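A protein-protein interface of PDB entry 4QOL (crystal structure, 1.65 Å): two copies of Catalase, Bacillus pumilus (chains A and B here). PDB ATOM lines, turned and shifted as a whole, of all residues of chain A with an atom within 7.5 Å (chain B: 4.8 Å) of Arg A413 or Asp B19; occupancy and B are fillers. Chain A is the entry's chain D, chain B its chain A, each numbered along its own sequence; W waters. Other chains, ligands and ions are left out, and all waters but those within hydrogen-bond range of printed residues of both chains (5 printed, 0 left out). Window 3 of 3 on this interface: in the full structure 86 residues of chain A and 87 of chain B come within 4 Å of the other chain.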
ATOM      1  N   ASP A 139     -25.357  16.565  11.219  1.00  0.00           N
ATOM      2  CA  ASP A 139     -25.606  15.211  11.617  1.00  0.00           C
ATOM      3  C   ASP A 139     -25.423  15.107  13.140  1.00  0.00           C
ATOM      4  O   ASP A 139     -24.423  15.544  13.668  1.00  0.00           O
ATOM      5  CB  ASP A 139     -24.653  14.247  10.869  1.00  0.00           C
ATOM      6  CG  ASP A 139     -25.049  12.789  11.027  1.00  0.00           C
ATOM      7  OD1 ASP A 139     -25.246  12.367  12.188  1.00  0.00           O
ATOM      8  OD2 ASP A 139     -25.197  12.081  10.006  1.00  0.00           O
ATOM      9  N   LEU A 141     -24.643  12.802  14.993  1.00  0.00           N
ATOM     10  CA  LEU A 141     -23.509  11.969  15.485  1.00  0.00           C
ATOM     11  C   LEU A 141     -22.389  12.894  15.920  1.00  0.00           C
ATOM     12  O   LEU A 141     -21.618  12.538  16.750  1.00  0.00           O
ATOM     13  CB  LEU A 141     -23.023  11.000  14.420  1.00  0.00           C
ATOM     14  CG  LEU A 141     -21.976   9.981  14.798  1.00  0.00           C
ATOM     15  CD1 LEU A 141     -22.421   9.130  15.972  1.00  0.00           C
ATOM     16  CD2 LEU A 141     -21.684   9.106  13.592  1.00  0.00           C
ATOM     17  N   LYS A 142     -22.322  14.109  15.359  1.00  0.00           N
ATOM     18  CA  LYS A 142     -21.239  15.037  15.703  1.00  0.00           C
ATOM     19  C   LYS A 142     -21.540  15.916  16.944  1.00  0.00           C
ATOM     20  O   LYS A 142     -20.676  16.643  17.367  1.00  0.00           O
ATOM     21  CB  LYS A 142     -20.936  15.976  14.526  1.00  0.00           C
ATOM     22  CG  LYS A 142     -20.500  15.298  13.237  1.00  0.00           C
ATOM     23  CD  LYS A 142     -19.463  14.183  13.498  1.00  0.00           C
ATOM     24  CE  LYS A 142     -18.232  14.697  14.153  1.00  0.00           C
ATOM     25  NZ  LYS A 142     -17.231  13.621  14.298  1.00  0.00           N
ATOM     26  N   LYS A 331     -30.786  15.169   9.316  1.00  0.00           N
ATOM     27  CA  LYS A 331     -30.108  14.174  10.157  1.00  0.00           C
ATOM     28  C   LYS A 331     -29.754  14.715  11.524  1.00  0.00           C
ATOM     29  O   LYS A 331     -29.473  13.951  12.434  1.00  0.00           O
ATOM     30  CB  LYS A 331     -28.837  13.578   9.532  1.00  0.00           C
ATOM     31  CG  LYS A 331     -29.034  12.889   8.217  1.00  0.00           C
ATOM     32  CD  LYS A 331     -27.729  12.329   7.631  1.00  0.00           C
ATOM     33  CE  LYS A 331     -27.869  11.938   6.174  1.00  0.00           C
ATOM     34  NZ  LYS A 331     -26.575  11.430   5.661  1.00  0.00           N
ATOM     35  N   ARG A 410     -30.799   1.540   0.371  1.00  0.00           N
ATOM     36  CA  ARG A 410     -29.915   0.837   1.302  1.00  0.00           C
ATOM     37  C   ARG A 410     -29.791   1.643   2.609  1.00  0.00           C
ATOM     38  O   ARG A 410     -29.910   2.863   2.595  1.00  0.00           O
ATOM     39  CB  ARG A 410     -28.525   0.643   0.691  1.00  0.00           C
ATOM     40  CG  ARG A 410     -28.438  -0.435  -0.389  1.00  0.00           C
ATOM     41  CD  ARG A 410     -26.971  -0.465  -0.843  1.00  0.00           C
ATOM     42  NE  ARG A 410     -26.437  -1.819  -0.990  1.00  0.00           N
ATOM     43  CZ  ARG A 410     -26.667  -2.637  -2.015  1.00  0.00           C
ATOM     44  NH1 ARG A 410     -26.109  -3.841  -2.041  1.00  0.00           N
ATOM     45  NH2 ARG A 410     -27.449  -2.266  -3.028  1.00  0.00           N
ATOM     46  N   MET A 411     -29.475   0.933   3.658  1.00  0.00           N
ATOM     47  CA  MET A 411     -29.012   1.524   4.896  1.00  0.00           C
ATOM     48  C   MET A 411     -27.567   1.938   4.726  1.00  0.00           C
ATOM     49  O   MET A 411     -26.686   1.096   4.570  1.00  0.00           O
ATOM     50  CB  MET A 411     -29.137   0.559   6.082  1.00  0.00           C
ATOM     51  CG  MET A 411     -30.440  -0.210   6.233  1.00  0.00           C
ATOM     52  SD  MET A 411     -30.391  -1.422   7.596  1.00  0.00           S
ATOM     53  CE  MET A 411     -30.683  -0.348   9.024  1.00  0.00           C
ATOM     54  N   VAL A 412     -27.305   3.234   4.801  1.00  0.00           N
ATOM     55  CA  VAL A 412     -25.971   3.763   4.553  1.00  0.00           C
ATOM     56  C   VAL A 412     -25.541   4.751   5.671  1.00  0.00           C
ATOM     57  O   VAL A 412     -26.393   5.371   6.305  1.00  0.00           O
ATOM     58  CB  VAL A 412     -25.849   4.410   3.185  1.00  0.00           C
ATOM     59  CG1 VAL A 412     -26.309   3.439   2.118  1.00  0.00           C
ATOM     60  CG2 VAL A 412     -26.636   5.727   3.126  1.00  0.00           C
ATOM     61  N   ARG A 413     -24.226   4.911   5.819  1.00  0.00           N
ATOM     62  CA  ARG A 413     -23.640   6.060   6.452  1.00  0.00           C
ATOM     63  C   ARG A 413     -22.859   6.869   5.449  1.00  0.00           C
ATOM     64  O   ARG A 413     -21.772   6.487   5.035  1.00  0.00           O
ATOM     65  CB  ARG A 413     -22.707   5.590   7.561  1.00  0.00           C
ATOM     66  CG  ARG A 413     -23.374   4.869   8.688  1.00  0.00           C
ATOM     67  CD  ARG A 413     -22.324   4.513   9.698  1.00  0.00           C
ATOM     68  NE  ARG A 413     -22.872   3.661  10.716  1.00  0.00           N
ATOM     69  CZ  ARG A 413     -23.394   4.060  11.864  1.00  0.00           C
ATOM     70  NH1 ARG A 413     -23.850   3.092  12.654  1.00  0.00           N
ATOM     71  NH2 ARG A 413     -23.477   5.380  12.234  1.00  0.00           N
ATOM     72  N   GLN A 414     -23.448   7.986   5.026  1.00  0.00           N
ATOM     73  CA  GLN A 414     -22.916   8.746   3.914  1.00  0.00           C
ATOM     74  C   GLN A 414     -23.408  10.192   4.002  1.00  0.00           C
ATOM     75  O   GLN A 414     -24.601  10.412   4.203  1.00  0.00           O
ATOM     76  CB  GLN A 414     -23.433   8.096   2.613  1.00  0.00           C
ATOM     77  CG  GLN A 414     -22.928   8.608   1.278  1.00  0.00           C
ATOM     78  CD  GLN A 414     -23.675   7.911   0.117  1.00  0.00           C
ATOM     79  OE1 GLN A 414     -24.220   6.816   0.282  1.00  0.00           O
ATOM     80  NE2 GLN A 414     -23.753   8.570  -1.017  1.00  0.00           N
ATOM     81  N   LYS A 415     -22.510  11.135   3.744  1.00  0.00           N
ATOM     82  CA  LYS A 415     -22.874  12.544   3.751  1.00  0.00           C
ATOM     83  C   LYS A 415     -23.934  12.814   2.685  1.00  0.00           C
ATOM     84  O   LYS A 415     -23.958  12.209   1.620  1.00  0.00           O
ATOM     85  CB  LYS A 415     -21.631  13.439   3.569  1.00  0.00           C
ATOM     86  CG  LYS A 415     -21.867  14.916   3.852  1.00  0.00           C
ATOM     87  CD  LYS A 415     -20.778  15.789   3.284  1.00  0.00           C
ATOM     88  CE  LYS A 415     -19.450  15.595   3.960  1.00  0.00           C
ATOM     89  NZ  LYS A 415     -18.504  16.580   3.374  1.00  0.00           N
ATOM     90  N   VAL B  17     -14.988   1.793  15.637  1.00  0.00           N
ATOM     91  CA  VAL B  17     -16.017   2.524  14.961  1.00  0.00           C
ATOM     92  C   VAL B  17     -15.614   2.733  13.479  1.00  0.00           C
ATOM     93  O   VAL B  17     -14.592   3.344  13.207  1.00  0.00           O
ATOM     94  CB  VAL B  17     -16.247   3.885  15.683  1.00  0.00           C
ATOM     95  CG1 VAL B  17     -17.055   4.874  14.834  1.00  0.00           C
ATOM     96  CG2 VAL B  17     -16.969   3.607  17.012  1.00  0.00           C
ATOM     97  N   GLY B  18     -16.450   2.266  12.563  1.00  0.00           N
ATOM     98  CA  GLY B  18     -16.193   2.479  11.143  1.00  0.00           C
ATOM     99  C   GLY B  18     -16.392   3.900  10.607  1.00  0.00           C
ATOM    100  O   GLY B  18     -15.703   4.332   9.656  1.00  0.00           O
ATOM    101  N   ASP B  19     -17.336   4.629  11.201  1.00  0.00           N
ATOM    102  CA  ASP B  19     -17.674   5.996  10.763  1.00  0.00           C
ATOM    103  C   ASP B  19     -18.185   6.798  11.966  1.00  0.00           C
ATOM    104  O   ASP B  19     -19.251   6.510  12.492  1.00  0.00           O
ATOM    105  CB  ASP B  19     -18.772   5.878   9.708  1.00  0.00           C
ATOM    106  CG  ASP B  19     -19.117   7.211   8.990  1.00  0.00           C
ATOM    107  OD1 ASP B  19     -18.813   8.306   9.449  1.00  0.00           O
ATOM    108  OD2 ASP B  19     -19.682   7.112   7.881  1.00  0.00           O
ATOM    109  N   ASN B  20     -17.404   7.804  12.359  1.00  0.00           N
ATOM    110  CA  ASN B  20     -17.779   8.665  13.425  1.00  0.00           C
ATOM    111  C   ASN B  20     -18.382   9.980  12.945  1.00  0.00           C
ATOM    112  O   ASN B  20     -18.461  10.906  13.758  1.00  0.00           O
ATOM    113  CB  ASN B  20     -16.574   8.902  14.337  1.00  0.00           C
ATOM    114  CG  ASN B  20     -16.948   9.554  15.691  1.00  0.00           C
ATOM    115  OD1 ASN B  20     -17.919   9.164  16.339  1.00  0.00           O
ATOM    116  ND2 ASN B  20     -16.173  10.531  16.089  1.00  0.00           N
ATOM    117  N   GLN B  21     -18.726  10.048  11.649  1.00  0.00           N
ATOM    118  CA  GLN B  21     -19.269  11.269  11.028  1.00  0.00           C
ATOM    119  C   GLN B  21     -20.724  11.200  10.673  1.00  0.00           C
ATOM    120  O   GLN B  21     -21.451  12.207  10.790  1.00  0.00           O
ATOM    121  CB  GLN B  21     -18.483  11.640   9.750  1.00  0.00           C
ATOM    122  CG  GLN B  21     -16.969  11.511   9.860  1.00  0.00           C
ATOM    123  CD  GLN B  21     -16.388  12.089  11.149  1.00  0.00           C
ATOM    124  OE1 GLN B  21     -16.758  13.211  11.577  1.00  0.00           O
ATOM    125  NE2 GLN B  21     -15.444  11.364  11.752  1.00  0.00           N
ATOM    126  N   ASN B  22     -21.176  10.043  10.153  1.00  0.00           N
ATOM    127  CA  ASN B  22     -22.533   9.946   9.587  1.00  0.00           C
ATOM    128  C   ASN B  22     -23.352   8.959  10.382  1.00  0.00           C
ATOM    129  O   ASN B  22     -22.905   7.812  10.626  1.00  0.00           O
ATOM    130  CB  ASN B  22     -22.489   9.499   8.114  1.00  0.00           C
ATOM    131  CG  ASN B  22     -21.590  10.384   7.269  1.00  0.00           C
ATOM    132  OD1 ASN B  22     -21.881  11.589   7.114  1.00  0.00           O
ATOM    133  ND2 ASN B  22     -20.432   9.863   6.891  1.00  0.00           N
ATOM    134  N   SER B  23     -24.552   9.367  10.740  1.00  0.00           N
ATOM    135  CA  SER B  23     -25.602   8.513  11.182  1.00  0.00           C
ATOM    136  C   SER B  23     -26.014   7.548  10.078  1.00  0.00           C
ATOM    137  O   SER B  23     -25.772   7.762   8.902  1.00  0.00           O
ATOM    138  CB  SER B  23     -26.858   9.326  11.558  1.00  0.00           C
ATOM    139  OG  SER B  23     -26.608  10.222  12.610  1.00  0.00           O
ATOM    140  N   ARG B  24     -26.643   6.453  10.499  1.00  0.00           N
ATOM    141  CA  ARG B  24     -27.129   5.479   9.547  1.00  0.00           C
ATOM    142  C   ARG B  24     -28.546   5.795   9.078  1.00  0.00           C
ATOM    143  O   ARG B  24     -29.468   5.947   9.900  1.00  0.00           O
ATOM    144  CB  ARG B  24     -27.040   4.099  10.233  1.00  0.00           C
ATOM    145  CG  ARG B  24     -27.164   2.950   9.337  1.00  0.00           C
ATOM    146  CD  ARG B  24     -27.017   1.667  10.148  1.00  0.00           C
ATOM    147  NE  ARG B  24     -26.677   0.579   9.243  1.00  0.00           N
ATOM    148  CZ  ARG B  24     -26.824  -0.697   9.544  1.00  0.00           C
ATOM    149  NH1 ARG B  24     -27.409  -1.046  10.710  1.00  0.00           N
ATOM    150  NH2 ARG B  24     -26.448  -1.595   8.663  1.00  0.00           N
ATOM    151  N   ASP B  36     -28.435   1.861  15.007  1.00  0.00           N
ATOM    152  CA  ASP B  36     -27.183   2.618  14.930  1.00  0.00           C
ATOM    153  C   ASP B  36     -26.671   2.668  16.345  1.00  0.00           C
ATOM    154  O   ASP B  36     -26.888   3.659  17.071  1.00  0.00           O
ATOM    155  CB  ASP B  36     -27.439   4.038  14.396  1.00  0.00           C
ATOM    156  CG  ASP B  36     -26.138   4.813  14.116  1.00  0.00           C
ATOM    157  OD1 ASP B  36     -25.076   4.391  14.608  1.00  0.00           O
ATOM    158  OD2 ASP B  36     -26.204   5.783  13.326  1.00  0.00           O
ATOM    159  N   HIS B  38     -23.727   2.871  17.677  1.00  0.00           N
ATOM    160  CA  HIS B  38     -22.769   3.914  17.972  1.00  0.00           C
ATOM    161  C   HIS B  38     -23.431   5.271  18.233  1.00  0.00           C
ATOM    162  O   HIS B  38     -23.090   5.964  19.197  1.00  0.00           O
ATOM    163  CB  HIS B  38     -21.729   4.047  16.840  1.00  0.00           C
ATOM    164  CG  HIS B  38     -20.726   5.167  17.032  1.00  0.00           C
ATOM    165  ND1 HIS B  38     -20.074   5.409  18.222  1.00  0.00           N
ATOM    166  CD2 HIS B  38     -20.214   6.059  16.163  1.00  0.00           C
ATOM    167  CE1 HIS B  38     -19.222   6.412  18.080  1.00  0.00           C
ATOM    168  NE2 HIS B  38     -19.332   6.867  16.862  1.00  0.00           N
HETATM  169  O   HOH W   1     -24.352  12.548   7.341  1.00  0.00           O
HETATM  170  O   HOH W   2     -22.866   1.214  15.345  1.00  0.00           O
HETATM  171  O   HOH W   3     -26.110   8.725   6.463  1.00  0.00           O
HETATM  172  O   HOH W   4     -29.317  11.153  13.084  1.00  0.00           O
HETATM  173  O   HOH W   5     -25.071   1.029   6.899  1.00  0.00           O
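No position is printed for both chains. Of the 20 pairs that touch across the chains among the printed residues, none has its exchanged pair printed and touching as well.
Water W3 lies within hydrogen-bond range of O of Ser B23, NZ of Lys A331, N of Gln A414 and O of Val A412. Water W1 lies within hydrogen-bond range of OD1 of Asn B22 (2.7 Å), OD2 of Asp A139 (2.8 Å) and NZ of Lys A331 (3.0 Å). Water W5 lies within hydrogen-bond range of O of Met A411 (2.8 Å) and NE of Arg B24 (2.9 Å). Water W4 lies within hydrogen-bond range of the backbone carbonyl oxygen (O) of Lys A331 (2.9 Å) and the side-chain hydroxyl (OG) of Ser B23 (2.9 Å). Water W2 bridges the backbone NH (N) of His B38 (3.0 Å) and the guanidinium group (NH1) of Arg A413 (3.4 Å).
The backbone NH (N) of Leu A141 is in hydrogen-bond range of the side-chain carboxylate (OD1) of Asp A139 (2.9 Å). The side-chain amide oxygen of Asn B20 sits at hydrogen-bond distance from a ring nitrogen (NE2) of His B38, 2.7 Å away. The backbone NH (N) of Asn B22 is in hydrogen-bond range of the side-chain carboxylate (OD1) of Asp B19 (3.0 Å). The backbone carbonyl oxygen (O) of Gln A414 lies within hydrogen-bond range of the side-chain amino group (NZ) of Lys A331 (2.7 Å). The side-chain carboxylate (OD1) of Asp B19 is in hydrogen-bond range of the backbone NH (N) of Gln B21. The backbone NH (N) of Arg B24 is in hydrogen-bond range of the side-chain carboxylate (OD2) of Asp B36 (2.9 Å).
Of the printed residues of chain B, Met A411 touches Arg B24 (3.7 Å). Of the printed residues of chain B, Val A412 touches Ser B23 and Arg B24. Of chain B, only Asp B19, Asn B22, Ser B23, Arg B24 and Asp B36 come within 4 Å of Arg A413. Printed residues of chain B within 4 Å of Gln A414: Asn B22 (3.6 Å). Asp B19 touches two residues of chain A. The nearest printed residue of chain B that does not touch Arg A413 is His B38 (4.8 Å). The nearest residue of chain A that does not touch Asp B19 is Gln A414 (4.8 Å).
Among the printed residues, merely in contact across the chains: Val A412 with Arg B24, Arg A413 with Asp B19, Asp A139 with Asn B22, Leu A141 with Asn B22, Leu A141 with Asn B20, Gln A414 with Asn B22, Val A412 with Ser B23, Asp A139 with Gln B21, Leu A141 with Gln B21, Arg A413 with Ser B23, Leu A141 with Asp B19, Met A411 with Arg B24, Arg A413 with Arg B24 and Leu A141 with His B38.
NZ of Lys A142 lies within hydrogen-bond range of O of Asn B20. The guanidinium group (NH2) of Arg A413 sits at hydrogen-bond distance from the backbone carbonyl oxygen (O) of Asn B22, 3.0 Å away. OG of Ser B23 is in hydrogen-bond range of OD1 of Asp A139, 2.6 Å away. NZ of Lys A142 lies within hydrogen-bond range of OE1 of Gln B21 (2.8 Å). OD1 of Asp B36 lies within salt-bridge range of NH1 of Arg A413. The side-chain amide oxygen (OD1) of Asn B22 lies within hydrogen-bond range of the backbone NH (N) of Lys A415, at 3.5 Å.
Printed residues of chain A that touch a printed residue of chain B: Asp A139, Leu A141, Lys A142, Met A411, Val A412, Arg A413, Gln A414 and Lys A415. Of the 10 printed residues of chain B, 8 touch a printed residue of chain A. Hydrophobic or aromatic side chains of chain B that line the printed part of chain A: His B38. Along chain B the printed residues that touch a printed residue of chain A span positions 19 to 38. Among the printed residues, 20 pairs touch across the chains. Among the printed residues, Asp or Glu carboxylates within 4 Å of a Lys or Arg side-chain nitrogen of the other chain: Arg A413 with Asp B36.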
